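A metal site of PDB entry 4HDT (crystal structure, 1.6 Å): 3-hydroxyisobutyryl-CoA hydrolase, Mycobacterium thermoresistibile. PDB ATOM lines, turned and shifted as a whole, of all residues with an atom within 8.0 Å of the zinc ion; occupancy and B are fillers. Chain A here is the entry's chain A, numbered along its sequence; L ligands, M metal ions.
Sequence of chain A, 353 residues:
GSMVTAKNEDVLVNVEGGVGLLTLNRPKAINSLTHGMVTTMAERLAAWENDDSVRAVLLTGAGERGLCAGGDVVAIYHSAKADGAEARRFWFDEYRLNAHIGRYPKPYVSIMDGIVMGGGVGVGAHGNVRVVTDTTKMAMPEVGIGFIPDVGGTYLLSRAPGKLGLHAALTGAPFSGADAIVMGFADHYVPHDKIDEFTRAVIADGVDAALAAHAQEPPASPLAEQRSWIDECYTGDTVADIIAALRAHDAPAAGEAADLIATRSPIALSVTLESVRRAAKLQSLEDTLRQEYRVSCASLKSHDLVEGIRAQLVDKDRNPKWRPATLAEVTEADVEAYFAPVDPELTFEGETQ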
ATOM      1  N   LEU A  45     -10.408 -10.362 -13.628  1.00  0.00           N
ATOM      2  CA  LEU A  45     -10.564  -9.561 -12.416  1.00  0.00           C
ATOM      3  C   LEU A  45      -9.322  -8.709 -12.149  1.00  0.00           C
ATOM      4  O   LEU A  45      -9.430  -7.534 -11.755  1.00  0.00           O
ATOM      5  CB  LEU A  45     -10.817 -10.443 -11.197  1.00  0.00           C
ATOM      6  CG  LEU A  45     -12.169 -11.118 -11.179  1.00  0.00           C
ATOM      7  CD1 LEU A  45     -12.245 -11.864  -9.869  1.00  0.00           C
ATOM      8  CD2 LEU A  45     -13.296 -10.102 -11.253  1.00  0.00           C
ATOM      9  N   ALA A  46      -8.147  -9.288 -12.345  1.00  0.00           N
ATOM     10  CA  ALA A  46      -6.924  -8.502 -12.163  1.00  0.00           C
ATOM     11  C   ALA A  46      -6.813  -7.349 -13.152  1.00  0.00           C
ATOM     12  O   ALA A  46      -6.411  -6.203 -12.783  1.00  0.00           O
ATOM     13  CB  ALA A  46      -5.701  -9.410 -12.272  1.00  0.00           C
ATOM     14  N   GLU A  49      -9.393  -4.497 -12.437  1.00  0.00           N
ATOM     15  CA  GLU A  49      -9.419  -3.903 -11.082  1.00  0.00           C
ATOM     16  C   GLU A  49      -9.089  -2.400 -11.066  1.00  0.00           C
ATOM     17  O   GLU A  49      -9.768  -1.607 -10.357  1.00  0.00           O
ATOM     18  CB  GLU A  49      -8.453  -4.651 -10.178  1.00  0.00           C
ATOM     19  CG  GLU A  49      -8.570  -4.301  -8.687  1.00  0.00           C
ATOM     20  CD  GLU A  49      -7.928  -5.336  -7.788  1.00  0.00           C
ATOM     21  OE1 GLU A  49      -7.240  -6.244  -8.313  1.00  0.00           O
ATOM     22  OE2 GLU A  49      -8.088  -5.276  -6.549  1.00  0.00           O
ATOM     23  N   ASN A  50      -8.065  -2.024 -11.826  1.00  0.00           N
ATOM     24  CA  ASN A  50      -7.620  -0.615 -11.896  1.00  0.00           C
ATOM     25  C   ASN A  50      -7.937   0.084 -13.236  1.00  0.00           C
ATOM     26  O   ASN A  50      -7.347   1.129 -13.575  1.00  0.00           O
ATOM     27  CB  ASN A  50      -6.122  -0.528 -11.585  1.00  0.00           C
ATOM     28  CG  ASN A  50      -5.789  -1.101 -10.224  1.00  0.00           C
ATOM     29  OD1 ASN A  50      -5.138  -2.139 -10.116  1.00  0.00           O
ATOM     30  ND2 ASN A  50      -6.268  -0.473  -9.190  1.00  0.00           N
ATOM     31  N   ALA A  99     -10.712 -15.809  -2.797  1.00  0.00           N
ATOM     32  CA  ALA A  99     -10.261 -14.714  -1.921  1.00  0.00           C
ATOM     33  C   ALA A  99     -10.304 -13.375  -2.597  1.00  0.00           C
ATOM     34  O   ALA A  99     -10.742 -12.375  -2.015  1.00  0.00           O
ATOM     35  CB  ALA A  99      -8.898 -15.024  -1.374  1.00  0.00           C
ATOM     36  N   HIS A 100      -9.850 -13.332  -3.847  1.00  0.00           N
ATOM     37  CA  HIS A 100      -9.900 -12.086  -4.572  1.00  0.00           C
ATOM     38  C   HIS A 100     -11.300 -11.548  -4.800  1.00  0.00           C
ATOM     39  O   HIS A 100     -11.551 -10.384  -4.610  1.00  0.00           O
ATOM     40  CB  HIS A 100      -9.183 -12.144  -5.896  1.00  0.00           C
ATOM     41  CG  HIS A 100      -8.714 -10.790  -6.339  1.00  0.00           C
ATOM     42  ND1 HIS A 100      -8.293 -10.526  -7.626  1.00  0.00           N
ATOM     43  CD2 HIS A 100      -8.603  -9.616  -5.658  1.00  0.00           C
ATOM     44  CE1 HIS A 100      -7.930  -9.257  -7.713  1.00  0.00           C
ATOM     45  NE2 HIS A 100      -8.098  -8.695  -6.524  1.00  0.00           N
ATOM     46  N   ILE A 101     -12.236 -12.408  -5.140  1.00  0.00           N
ATOM     47  CA  ILE A 101     -13.651 -11.993  -5.223  1.00  0.00           C
ATOM     48  C   ILE A 101     -14.118 -11.449  -3.888  1.00  0.00           C
ATOM     49  O   ILE A 101     -14.783 -10.400  -3.842  1.00  0.00           O
ATOM     50  CB  ILE A 101     -14.538 -13.180  -5.667  1.00  0.00           C
ATOM     51  CG1 ILE A 101     -14.131 -13.684  -7.077  1.00  0.00           C
ATOM     52  CG2 ILE A 101     -16.007 -12.767  -5.648  1.00  0.00           C
ATOM     53  CD1 ILE A 101     -14.600 -15.123  -7.365  1.00  0.00           C
ATOM     54  N   ARG A 103     -12.366  -9.938  -1.494  1.00  0.00           N
ATOM     55  CA  ARG A 103     -11.767  -8.615  -1.284  1.00  0.00           C
ATOM     56  C   ARG A 103     -12.130  -7.566  -2.306  1.00  0.00           C
ATOM     57  O   ARG A 103     -11.746  -6.398  -2.169  1.00  0.00           O
ATOM     58  CB  ARG A 103     -10.228  -8.753  -1.453  1.00  0.00           C
ATOM     59  CG  ARG A 103      -9.601  -9.511  -0.357  1.00  0.00           C
ATOM     60  CD  ARG A 103      -8.088  -9.336  -0.376  1.00  0.00           C
ATOM     61  NE  ARG A 103      -7.422  -9.520  -1.673  1.00  0.00           N
ATOM     62  CZ  ARG A 103      -7.031 -10.704  -2.189  1.00  0.00           C
ATOM     63  NH1 ARG A 103      -7.204 -11.847  -1.532  1.00  0.00           N
ATOM     64  NH2 ARG A 103      -6.445 -10.746  -3.345  1.00  0.00           N
ATOM     65  N   TYR A 104     -12.702  -7.991  -3.433  1.00  0.00           N
ATOM     66  CA  TYR A 104     -12.685  -7.142  -4.630  1.00  0.00           C
ATOM     67  C   TYR A 104     -13.256  -5.719  -4.365  1.00  0.00           C
ATOM     68  O   TYR A 104     -14.312  -5.559  -3.741  1.00  0.00           O
ATOM     69  CB  TYR A 104     -13.470  -7.776  -5.756  1.00  0.00           C
ATOM     70  CG  TYR A 104     -12.989  -7.405  -7.176  1.00  0.00           C
ATOM     71  CD1 TYR A 104     -11.698  -7.675  -7.599  1.00  0.00           C
ATOM     72  CD2 TYR A 104     -13.831  -6.732  -8.059  1.00  0.00           C
ATOM     73  CE1 TYR A 104     -11.252  -7.324  -8.847  1.00  0.00           C
ATOM     74  CE2 TYR A 104     -13.429  -6.393  -9.323  1.00  0.00           C
ATOM     75  CZ  TYR A 104     -12.128  -6.692  -9.742  1.00  0.00           C
ATOM     76  OH  TYR A 104     -11.687  -6.348 -10.996  1.00  0.00           O
ATOM     77  N   PRO A 105     -12.533  -4.689  -4.789  1.00  0.00           N
ATOM     78  CA  PRO A 105     -12.951  -3.335  -4.449  1.00  0.00           C
ATOM     79  C   PRO A 105     -14.192  -2.842  -5.197  1.00  0.00           C
ATOM     80  O   PRO A 105     -14.982  -2.043  -4.619  1.00  0.00           O
ATOM     81  CB  PRO A 105     -11.692  -2.505  -4.722  1.00  0.00           C
ATOM     82  CG  PRO A 105     -10.962  -3.258  -5.776  1.00  0.00           C
ATOM     83  CD  PRO A 105     -11.212  -4.705  -5.460  1.00  0.00           C
ATOM     84  N   LYS A 106     -14.458  -3.368  -6.400  1.00  0.00           N
ATOM     85  CA  LYS A 106     -15.584  -2.927  -7.228  1.00  0.00           C
ATOM     86  C   LYS A 106     -16.804  -3.856  -7.004  1.00  0.00           C
ATOM     87  O   LYS A 106     -16.644  -4.983  -6.624  1.00  0.00           O
ATOM     88  CB  LYS A 106     -15.167  -2.921  -8.698  1.00  0.00           C
ATOM     89  CG  LYS A 106     -14.079  -1.884  -8.973  1.00  0.00           C
ATOM     90  CD  LYS A 106     -13.563  -1.975 -10.408  1.00  0.00           C
ATOM     91  CE  LYS A 106     -12.678  -0.791 -10.711  1.00  0.00           C
ATOM     92  NZ  LYS A 106     -12.080  -0.749 -12.089  1.00  0.00           N
ATOM     93  N   GLY A 350       1.108 -11.411  -4.928  1.00  0.00           N
ATOM     94  CA  GLY A 350       0.968 -11.180  -6.385  1.00  0.00           C
ATOM     95  C   GLY A 350      -0.198 -10.274  -6.803  1.00  0.00           C
ATOM     96  O   GLY A 350      -0.617 -10.240  -7.974  1.00  0.00           O
ATOM     97  N   GLU A 351      -0.759  -9.542  -5.843  1.00  0.00           N
ATOM     98  CA  GLU A 351      -1.909  -8.694  -6.076  1.00  0.00           C
ATOM     99  C   GLU A 351      -1.647  -7.611  -7.157  1.00  0.00           C
ATOM    100  O   GLU A 351      -0.535  -7.093  -7.273  1.00  0.00           O
ATOM    101  CB  GLU A 351      -2.307  -8.080  -4.721  1.00  0.00           C
ATOM    102  CG  GLU A 351      -3.320  -6.975  -4.770  1.00  0.00           C
ATOM    103  CD  GLU A 351      -4.700  -7.438  -5.142  1.00  0.00           C
ATOM    104  OE1 GLU A 351      -5.397  -6.604  -5.726  1.00  0.00           O
ATOM    105  OE2 GLU A 351      -5.065  -8.597  -4.846  1.00  0.00           O
HETATM  106 CL1  LIG L   1      -8.075  -6.764  -3.583  1.00  0.00          CL
HETATM  107 ZN    ZN M   1      -7.383  -6.888  -5.754  1.00  0.00          ZN
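The backbone NH (N) of Glu 49 is in hydrogen-bond range of the side-chain hydroxyl (OH) of Tyr 104 (3.3 Å).
OE2 of Glu 351 is in salt-bridge range of NH2 of Arg 103 (3.0 Å).
NZ of Lys 106 lies within hydrogen-bond range of O of Glu 49 (3.0 Å).
Within 4 Å of the zinc ion: Glu 49, His 100 and Glu 351.
The zinc ion is bound by OE2 of Glu 49 (1.9 Å), OE1 of Glu 351 (2.0 Å), NE2 of His 100 (2.1 Å) and CL1 of the ligand (2.3 Å).
The zinc ion has four donor atoms within binding distance.
Slightly farther from the zinc ion lies OE1 of Glu 49 (2.6 Å).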
